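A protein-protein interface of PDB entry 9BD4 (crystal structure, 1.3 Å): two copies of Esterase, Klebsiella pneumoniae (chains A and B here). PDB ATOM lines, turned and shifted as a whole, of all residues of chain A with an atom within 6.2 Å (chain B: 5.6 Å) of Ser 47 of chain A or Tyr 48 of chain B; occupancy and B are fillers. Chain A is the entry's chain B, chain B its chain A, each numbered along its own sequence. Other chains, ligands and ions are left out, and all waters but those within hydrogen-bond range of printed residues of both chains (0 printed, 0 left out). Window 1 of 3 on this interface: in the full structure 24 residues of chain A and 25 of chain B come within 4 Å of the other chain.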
ATOM      1  N   LEU A   7      -8.615 -16.631 -12.292  1.00  0.00           N
ATOM      2  CA  LEU A   7      -9.629 -16.267 -11.316  1.00  0.00           C
ATOM      3  C   LEU A   7     -10.928 -16.963 -11.690  1.00  0.00           C
ATOM      4  O   LEU A   7     -11.318 -16.986 -12.859  1.00  0.00           O
ATOM      5  CB  LEU A   7      -9.804 -14.737 -11.246  1.00  0.00           C
ATOM      6  CG  LEU A   7     -10.712 -14.117 -10.184  1.00  0.00           C
ATOM      7  CD1 LEU A   7     -10.281 -12.685  -9.916  1.00  0.00           C
ATOM      8  CD2 LEU A   7     -12.176 -14.148 -10.606  1.00  0.00           C
ATOM      9  N   LEU A  18     -14.838 -16.408  -4.497  1.00  0.00           N
ATOM     10  CA  LEU A  18     -13.947 -15.998  -5.566  1.00  0.00           C
ATOM     11  C   LEU A  18     -12.547 -16.497  -5.224  1.00  0.00           C
ATOM     12  O   LEU A  18     -12.071 -16.309  -4.096  1.00  0.00           O
ATOM     13  CB  LEU A  18     -13.976 -14.474  -5.712  1.00  0.00           C
ATOM     14  CG  LEU A  18     -13.160 -13.841  -6.838  1.00  0.00           C
ATOM     15  CD1 LEU A  18     -13.797 -12.522  -7.237  1.00  0.00           C
ATOM     16  CD2 LEU A  18     -11.712 -13.627  -6.437  1.00  0.00           C
ATOM     17  N   SER A  42     -19.209  -6.081  -2.162  1.00  0.00           N
ATOM     18  CA  SER A  42     -19.231  -7.494  -2.502  1.00  0.00           C
ATOM     19  C   SER A  42     -17.814  -7.969  -2.775  1.00  0.00           C
ATOM     20  O   SER A  42     -16.888  -7.168  -2.960  1.00  0.00           O
ATOM     21  CB  SER A  42     -20.109  -7.760  -3.724  1.00  0.00           C
ATOM     22  OG  SER A  42     -19.463  -7.311  -4.915  1.00  0.00           O
ATOM     23  N   LYS A  43     -17.669  -9.294  -2.848  1.00  0.00           N
ATOM     24  CA  LYS A  43     -16.370  -9.864  -3.178  1.00  0.00           C
ATOM     25  C   LYS A  43     -15.935  -9.470  -4.584  1.00  0.00           C
ATOM     26  O   LYS A  43     -14.735  -9.344  -4.843  1.00  0.00           O
ATOM     27  CB  LYS A  43     -16.389 -11.389  -3.015  1.00  0.00           C
ATOM     28  CG  LYS A  43     -17.348 -12.128  -3.943  1.00  0.00           C
ATOM     29  CD  LYS A  43     -17.415 -13.611  -3.550  1.00  0.00           C
ATOM     30  CE  LYS A  43     -18.199 -14.455  -4.537  1.00  0.00           C
ATOM     31  NZ  LYS A  43     -19.615 -14.012  -4.704  1.00  0.00           N
ATOM     32  N   LEU A  44     -16.881  -9.256  -5.499  1.00  0.00           N
ATOM     33  CA  LEU A  44     -16.511  -8.847  -6.849  1.00  0.00           C
ATOM     34  C   LEU A  44     -15.980  -7.415  -6.868  1.00  0.00           C
ATOM     35  O   LEU A  44     -14.981  -7.130  -7.538  1.00  0.00           O
ATOM     36  CB  LEU A  44     -17.711  -9.003  -7.793  1.00  0.00           C
ATOM     37  CG  LEU A  44     -17.458  -8.721  -9.271  1.00  0.00           C
ATOM     38  CD1 LEU A  44     -16.402  -9.685  -9.826  1.00  0.00           C
ATOM     39  CD2 LEU A  44     -18.757  -8.841 -10.069  1.00  0.00           C
ATOM     40  N   VAL A  45     -16.625  -6.502  -6.135  1.00  0.00           N
ATOM     41  CA  VAL A  45     -16.156  -5.116  -6.090  1.00  0.00           C
ATOM     42  C   VAL A  45     -14.779  -5.031  -5.436  1.00  0.00           C
ATOM     43  O   VAL A  45     -13.968  -4.163  -5.800  1.00  0.00           O
ATOM     44  CB  VAL A  45     -17.213  -4.218  -5.410  1.00  0.00           C
ATOM     45  CG1 VAL A  45     -16.684  -2.811  -5.127  1.00  0.00           C
ATOM     46  CG2 VAL A  45     -18.451  -4.158  -6.270  1.00  0.00           C
ATOM     47  N   TYR A  46     -14.478  -5.924  -4.486  1.00  0.00           N
ATOM     48  CA  TYR A  46     -13.177  -5.936  -3.823  1.00  0.00           C
ATOM     49  C   TYR A  46     -12.189  -6.902  -4.478  1.00  0.00           C
ATOM     50  O   TYR A  46     -11.114  -7.154  -3.913  1.00  0.00           O
ATOM     51  CB  TYR A  46     -13.331  -6.213  -2.316  1.00  0.00           C
ATOM     52  CG  TYR A  46     -13.527  -4.947  -1.498  1.00  0.00           C
ATOM     53  CD1 TYR A  46     -14.801  -4.418  -1.265  1.00  0.00           C
ATOM     54  CD2 TYR A  46     -12.433  -4.266  -0.978  1.00  0.00           C
ATOM     55  CE1 TYR A  46     -14.970  -3.248  -0.507  1.00  0.00           C
ATOM     56  CE2 TYR A  46     -12.594  -3.107  -0.227  1.00  0.00           C
ATOM     57  CZ  TYR A  46     -13.853  -2.612   0.013  1.00  0.00           C
ATOM     58  OH  TYR A  46     -13.973  -1.459   0.770  1.00  0.00           O
ATOM     59  N   SER A  47     -12.514  -7.435  -5.662  1.00  0.00           N
ATOM     60  CA  SER A  47     -11.684  -8.481  -6.268  1.00  0.00           C
ATOM     61  C   SER A  47     -10.321  -7.967  -6.721  1.00  0.00           C
ATOM     62  O   SER A  47      -9.444  -8.789  -7.024  1.00  0.00           O
ATOM     63  CB  SER A  47     -12.403  -9.149  -7.450  1.00  0.00           C
ATOM     64  OG  SER A  47     -12.688  -8.234  -8.491  1.00  0.00           O
ATOM     65  N   TYR A  48     -10.120  -6.647  -6.764  1.00  0.00           N
ATOM     66  CA  TYR A  48      -8.790  -6.124  -7.060  1.00  0.00           C
ATOM     67  C   TYR A  48      -7.761  -6.569  -6.016  1.00  0.00           C
ATOM     68  O   TYR A  48      -6.569  -6.656  -6.337  1.00  0.00           O
ATOM     69  CB  TYR A  48      -8.840  -4.601  -7.221  1.00  0.00           C
ATOM     70  CG  TYR A  48      -9.244  -3.839  -5.981  1.00  0.00           C
ATOM     71  CD1 TYR A  48     -10.591  -3.630  -5.665  1.00  0.00           C
ATOM     72  CD2 TYR A  48      -8.276  -3.273  -5.156  1.00  0.00           C
ATOM     73  CE1 TYR A  48     -10.955  -2.920  -4.519  1.00  0.00           C
ATOM     74  CE2 TYR A  48      -8.626  -2.553  -4.025  1.00  0.00           C
ATOM     75  CZ  TYR A  48      -9.963  -2.381  -3.713  1.00  0.00           C
ATOM     76  OH  TYR A  48     -10.328  -1.658  -2.594  1.00  0.00           O
ATOM     77  N   PHE A  49      -8.177  -6.825  -4.767  1.00  0.00           N
ATOM     78  CA  PHE A  49      -7.239  -7.389  -3.793  1.00  0.00           C
ATOM     79  C   PHE A  49      -6.776  -8.777  -4.213  1.00  0.00           C
ATOM     80  O   PHE A  49      -5.602  -9.131  -4.024  1.00  0.00           O
ATOM     81  CB  PHE A  49      -7.859  -7.431  -2.393  1.00  0.00           C
ATOM     82  CG  PHE A  49      -7.698  -6.150  -1.624  1.00  0.00           C
ATOM     83  CD1 PHE A  49      -6.545  -5.895  -0.889  1.00  0.00           C
ATOM     84  CD2 PHE A  49      -8.694  -5.193  -1.657  1.00  0.00           C
ATOM     85  CE1 PHE A  49      -6.394  -4.711  -0.190  1.00  0.00           C
ATOM     86  CE2 PHE A  49      -8.562  -4.014  -0.963  1.00  0.00           C
ATOM     87  CZ  PHE A  49      -7.405  -3.764  -0.227  1.00  0.00           C
ATOM     88  N   ALA A  50      -7.692  -9.586  -4.753  1.00  0.00           N
ATOM     89  CA  ALA A  50      -7.326 -10.909  -5.245  1.00  0.00           C
ATOM     90  C   ALA A  50      -6.382 -10.813  -6.437  1.00  0.00           C
ATOM     91  O   ALA A  50      -5.425 -11.587  -6.534  1.00  0.00           O
ATOM     92  CB  ALA A  50      -8.580 -11.715  -5.592  1.00  0.00           C
ATOM     93  N   VAL A  51      -6.629  -9.874  -7.355  1.00  0.00           N
ATOM     94  CA  VAL A  51      -5.717  -9.658  -8.474  1.00  0.00           C
ATOM     95  C   VAL A  51      -4.328  -9.285  -7.968  1.00  0.00           C
ATOM     96  O   VAL A  51      -3.320  -9.889  -8.358  1.00  0.00           O
ATOM     97  CB  VAL A  51      -6.278  -8.590  -9.430  1.00  0.00           C
ATOM     98  CG1 VAL A  51      -5.284  -8.300 -10.540  1.00  0.00           C
ATOM     99  CG2 VAL A  51      -7.630  -9.047 -10.021  1.00  0.00           C
ATOM    100  N   ALA A  52      -4.256  -8.279  -7.094  1.00  0.00           N
ATOM    101  CA  ALA A  52      -2.961  -7.787  -6.633  1.00  0.00           C
ATOM    102  C   ALA A  52      -2.183  -8.857  -5.875  1.00  0.00           C
ATOM    103  O   ALA A  52      -0.977  -9.024  -6.089  1.00  0.00           O
ATOM    104  CB  ALA A  52      -3.175  -6.573  -5.734  1.00  0.00           C
ATOM    105  N   MET A  62     -11.986 -15.229  -1.488  1.00  0.00           N
ATOM    106  CA  MET A  62     -12.903 -14.170  -1.059  1.00  0.00           C
ATOM    107  C   MET A  62     -14.327 -14.677  -0.924  1.00  0.00           C
ATOM    108  O   MET A  62     -14.940 -15.056  -1.941  1.00  0.00           O
ATOM    109  CB  MET A  62     -12.857 -12.941  -1.968  1.00  0.00           C
ATOM    110  CG  MET A  62     -11.481 -12.335  -2.068  1.00  0.00           C
ATOM    111  SD  MET A  62     -11.348 -10.927  -3.163  1.00  0.00           S
ATOM    112  CE  MET A  62     -12.334  -9.765  -2.235  1.00  0.00           C
ATOM    113  N   LEU B  44      -4.735  -1.209 -11.395  1.00  0.00           N
ATOM    114  CA  LEU B  44      -4.854  -2.345 -10.488  1.00  0.00           C
ATOM    115  C   LEU B  44      -5.992  -2.143  -9.483  1.00  0.00           C
ATOM    116  O   LEU B  44      -6.767  -3.074  -9.216  1.00  0.00           O
ATOM    117  CB  LEU B  44      -3.523  -2.585  -9.786  1.00  0.00           C
ATOM    118  CG  LEU B  44      -3.428  -3.796  -8.858  1.00  0.00           C
ATOM    119  CD1 LEU B  44      -3.691  -5.107  -9.605  1.00  0.00           C
ATOM    120  CD2 LEU B  44      -2.059  -3.837  -8.174  1.00  0.00           C
ATOM    121  N   VAL B  45      -6.131  -0.931  -8.936  1.00  0.00           N
ATOM    122  CA  VAL B  45      -7.208  -0.676  -7.980  1.00  0.00           C
ATOM    123  C   VAL B  45      -8.576  -0.809  -8.650  1.00  0.00           C
ATOM    124  O   VAL B  45      -9.549  -1.241  -8.015  1.00  0.00           O
ATOM    125  CB  VAL B  45      -6.996   0.689  -7.284  1.00  0.00           C
ATOM    126  CG1 VAL B  45      -8.202   1.086  -6.422  1.00  0.00           C
ATOM    127  CG2 VAL B  45      -5.760   0.665  -6.405  1.00  0.00           C
ATOM    128  N   TYR B  46      -8.679  -0.469  -9.943  1.00  0.00           N
ATOM    129  CA  TYR B  46      -9.935  -0.575 -10.683  1.00  0.00           C
ATOM    130  C   TYR B  46     -10.063  -1.902 -11.438  1.00  0.00           C
ATOM    131  O   TYR B  46     -10.992  -2.063 -12.240  1.00  0.00           O
ATOM    132  CB  TYR B  46     -10.099   0.620 -11.642  1.00  0.00           C
ATOM    133  CG  TYR B  46     -10.811   1.800 -11.010  1.00  0.00           C
ATOM    134  CD1 TYR B  46     -12.190   1.906 -11.067  1.00  0.00           C
ATOM    135  CD2 TYR B  46     -10.104   2.797 -10.327  1.00  0.00           C
ATOM    136  CE1 TYR B  46     -12.857   2.983 -10.481  1.00  0.00           C
ATOM    137  CE2 TYR B  46     -10.767   3.887  -9.749  1.00  0.00           C
ATOM    138  CZ  TYR B  46     -12.141   3.956  -9.827  1.00  0.00           C
ATOM    139  OH  TYR B  46     -12.820   5.023  -9.268  1.00  0.00           O
ATOM    140  N   SER B  47      -9.180  -2.874 -11.177  1.00  0.00           N
ATOM    141  CA  SER B  47      -9.181  -4.119 -11.948  1.00  0.00           C
ATOM    142  C   SER B  47     -10.416  -4.983 -11.705  1.00  0.00           C
ATOM    143  O   SER B  47     -10.649  -5.927 -12.476  1.00  0.00           O
ATOM    144  CB  SER B  47      -7.910  -4.936 -11.658  1.00  0.00           C
ATOM    145  OG  SER B  47      -7.840  -5.349 -10.300  1.00  0.00           O
ATOM    146  N   TYR B  48     -11.213  -4.688 -10.681  1.00  0.00           N
ATOM    147  CA  TYR B  48     -12.484  -5.387 -10.509  1.00  0.00           C
ATOM    148  C   TYR B  48     -13.428  -5.200 -11.702  1.00  0.00           C
ATOM    149  O   TYR B  48     -14.276  -6.064 -11.957  1.00  0.00           O
ATOM    150  CB  TYR B  48     -13.127  -4.982  -9.178  1.00  0.00           C
ATOM    151  CG  TYR B  48     -13.540  -3.526  -9.091  1.00  0.00           C
ATOM    152  CD1 TYR B  48     -12.634  -2.546  -8.698  1.00  0.00           C
ATOM    153  CD2 TYR B  48     -14.856  -3.147  -9.345  1.00  0.00           C
ATOM    154  CE1 TYR B  48     -13.014  -1.205  -8.601  1.00  0.00           C
ATOM    155  CE2 TYR B  48     -15.254  -1.814  -9.230  1.00  0.00           C
ATOM    156  CZ  TYR B  48     -14.334  -0.855  -8.864  1.00  0.00           C
ATOM    157  OH  TYR B  48     -14.716   0.474  -8.737  1.00  0.00           O
ATOM    158  N   PHE B  49     -13.335  -4.074 -12.424  1.00  0.00           N
ATOM    159  CA  PHE B  49     -14.096  -3.943 -13.661  1.00  0.00           C
ATOM    160  C   PHE B  49     -13.646  -4.963 -14.695  1.00  0.00           C
ATOM    161  O   PHE B  49     -14.477  -5.527 -15.425  1.00  0.00           O
ATOM    162  CB  PHE B  49     -13.982  -2.525 -14.222  1.00  0.00           C
ATOM    163  CG  PHE B  49     -14.985  -1.558 -13.650  1.00  0.00           C
ATOM    164  CD1 PHE B  49     -16.266  -1.448 -14.196  1.00  0.00           C
ATOM    165  CD2 PHE B  49     -14.642  -0.737 -12.577  1.00  0.00           C
ATOM    166  CE1 PHE B  49     -17.179  -0.550 -13.676  1.00  0.00           C
ATOM    167  CE2 PHE B  49     -15.553   0.164 -12.053  1.00  0.00           C
ATOM    168  CZ  PHE B  49     -16.825   0.260 -12.610  1.00  0.00           C
ATOM    169  N   ALA B  50     -12.334  -5.194 -14.796  1.00  0.00           N
ATOM    170  CA  ALA B  50     -11.839  -6.205 -15.725  1.00  0.00           C
ATOM    171  C   ALA B  50     -12.324  -7.591 -15.318  1.00  0.00           C
ATOM    172  O   ALA B  50     -12.703  -8.399 -16.175  1.00  0.00           O
ATOM    173  CB  ALA B  50     -10.309  -6.140 -15.804  1.00  0.00           C
ATOM    174  N   VAL B  51     -12.324  -7.883 -14.017  1.00  0.00           N
ATOM    175  CA  VAL B  51     -12.828  -9.174 -13.548  1.00  0.00           C
ATOM    176  C   VAL B  51     -14.289  -9.349 -13.943  1.00  0.00           C
ATOM    177  O   VAL B  51     -14.675 -10.362 -14.537  1.00  0.00           O
ATOM    178  CB  VAL B  51     -12.623  -9.310 -12.027  1.00  0.00           C
ATOM    179  CG1 VAL B  51     -13.297 -10.580 -11.502  1.00  0.00           C
ATOM    180  CG2 VAL B  51     -11.128  -9.292 -11.692  1.00  0.00           C
ATOM    181  N   ALA B  52     -15.123  -8.356 -13.617  1.00  0.00           N
ATOM    182  CA  ALA B  52     -16.558  -8.490 -13.845  1.00  0.00           C
ATOM    183  C   ALA B  52     -16.877  -8.589 -15.332  1.00  0.00           C
ATOM    184  O   ALA B  52     -17.734  -9.384 -15.734  1.00  0.00           O
ATOM    185  CB  ALA B  52     -17.290  -7.300 -13.221  1.00  0.00           C
ATOM    186  N   LEU B  53     -16.205  -7.785 -16.161  1.00  0.00           N
ATOM    187  CA  LEU B  53     -16.523  -7.777 -17.585  1.00  0.00           C
ATOM    188  C   LEU B  53     -15.984  -9.023 -18.286  1.00  0.00           C
ATOM    189  O   LEU B  53     -16.650  -9.573 -19.178  1.00  0.00           O
ATOM    190  CB  LEU B  53     -16.050  -6.474 -18.221  1.00  0.00           C
ATOM    191  CG  LEU B  53     -16.951  -5.300 -17.800  1.00  0.00           C
ATOM    192  CD1 LEU B  53     -16.239  -3.990 -18.051  1.00  0.00           C
ATOM    193  CD2 LEU B  53     -18.314  -5.326 -18.500  1.00  0.00           C
ATOM    194  N   ILE B 225     -18.080   3.283  -6.459  1.00  0.00           N
ATOM    195  CA  ILE B 225     -18.730   2.282  -7.299  1.00  0.00           C
ATOM    196  C   ILE B 225     -19.293   1.174  -6.412  1.00  0.00           C
ATOM    197  O   ILE B 225     -18.569   0.549  -5.632  1.00  0.00           O
ATOM    198  CB  ILE B 225     -17.742   1.709  -8.323  1.00  0.00           C
ATOM    199  CG1 ILE B 225     -17.149   2.824  -9.198  1.00  0.00           C
ATOM    200  CG2 ILE B 225     -18.421   0.643  -9.171  1.00  0.00           C
ATOM    201  CD1 ILE B 225     -18.182   3.615  -9.992  1.00  0.00           C
ATOM    202  N   LEU B 230     -21.695  -1.755 -10.773  1.00  0.00           N
ATOM    203  CA  LEU B 230     -20.937  -2.732 -11.532  1.00  0.00           C
ATOM    204  C   LEU B 230     -21.868  -3.632 -12.335  1.00  0.00           C
ATOM    205  O   LEU B 230     -21.636  -3.856 -13.532  1.00  0.00           O
ATOM    206  CB  LEU B 230     -20.040  -3.510 -10.567  1.00  0.00           C
ATOM    207  CG  LEU B 230     -19.059  -4.481 -11.212  1.00  0.00           C
ATOM    208  CD1 LEU B 230     -18.072  -3.753 -12.115  1.00  0.00           C
ATOM    209  CD2 LEU B 230     -18.332  -5.225 -10.114  1.00  0.00           C
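Among the printed residues, merely in contact across the chains: Leu 7 of chain A with Val 51 of chain B (3.8 Å), Leu 44 of chain A with Tyr 48 of chain B (3.3 Å), Leu 44 of chain A with Val 51 of chain B (3.6 Å), Leu 44 of chain A with Ala 52 of chain B (3.8 Å), Leu 44 of chain A with Leu 230 of chain B (3.6 Å), Val 45 of chain A with Tyr 48 of chain B (3.4 Å), Val 45 of chain A with Ile 225 of chain B (3.9 Å), Val 45 of chain A with Leu 230 of chain B (3.99 Å), Ser 47 of chain A with Tyr 48 of chain B (3.4 Å), Ser 47 of chain A with Val 51 of chain B (3.7 Å), Tyr 48 of chain A with Leu 44 of chain B (3.3 Å), Tyr 48 of chain A with Val 45 of chain B (3.3 Å), Tyr 48 of chain A with Ser 47 of chain B (3.3 Å), Tyr 48 of chain A with Tyr 48 of chain B (3.8 Å), Val 51 of chain A with Leu 44 of chain B (3.7 Å), Val 51 of chain A with Ser 47 of chain B (3.7 Å), Val 51 of chain A with Val 51 of chain B (3.9 Å) and Ala 52 of chain A with Leu 44 of chain B (3.8 Å).
Of chain B, only Tyr 48 and Val 51 come within 4 Å of Ser 47 of chain A. Of chain A, only Leu 44 (3.3 Å), Val 45 (3.4 Å), Ser 47 (3.4 Å) and Tyr 48 (3.8 Å) come within 4 Å of Tyr 48 of chain B. Printed residues of chain B within 4 Å of Ala 52 of chain A: Leu 44 (3.8 Å). Of the printed residues of chain A, Ser 47 of chain B touches Tyr 48 and Val 51. Of the printed residues of chain B, Leu 7 of chain A touches Val 51. Leu 18 of chain A touches none of the printed residues of chain B. The nearest residue of chain B that does not touch Ser 47 of chain A is Ser 47 of chain B (5.0 Å). The nearest printed residue of chain B that does not touch Val 45 of chain A is Val 45 of chain B (5.7 Å).
Along chain A the printed residues that touch a printed residue of chain B span positions 7 to 52. Of the 12 printed residues of chain B, 8 touch a printed residue of chain A. Hydrophobic or aromatic side chains of chain B that line the printed part of chain A: Leu 44, Tyr 48, Val 51, Ala 52 and Leu 230. Among the printed residues, no Asp or Glu carboxylate lies within 4 Å of a Lys or Arg side-chain nitrogen of the other chain.
The side-chain hydroxyl of Ser 47 of chain A lies within hydrogen-bond range of the backbone carbonyl oxygen of Leu 44 of chain A, 2.7 Å away. The side-chain hydroxyl (OG) of Ser 42 of chain A lies within hydrogen-bond range of the backbone NH (N) of Val 45 of chain A. The side-chain hydroxyl of Ser 42 of chain A sits close to the backbone NH of Leu 44 of chain A, 3.3 Å away. The side-chain hydroxyl of Ser 47 of chain B lies within hydrogen-bond range of the backbone carbonyl oxygen of Leu 44 of chain B (2.7 Å).
Leu 44 of chain A touches Tyr 48 of chain B, and with the chains exchanged Tyr 48 of chain A touches Leu 44 of chain B. Leu 44 of chain A touches Val 51 of chain B, and with the chains exchanged Val 51 of chain A touches Leu 44 of chain B. Ser 47 of chain A touches Tyr 48 of chain B, and with the chains exchanged Tyr 48 of chain A touches Ser 47 of chain B. Val 51 of chain A touches its own counterpart, Val 51 of chain B. Of the 18 pairs that touch across the chains among the printed residues, 14 have their exchanged pair printed and touching as well.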
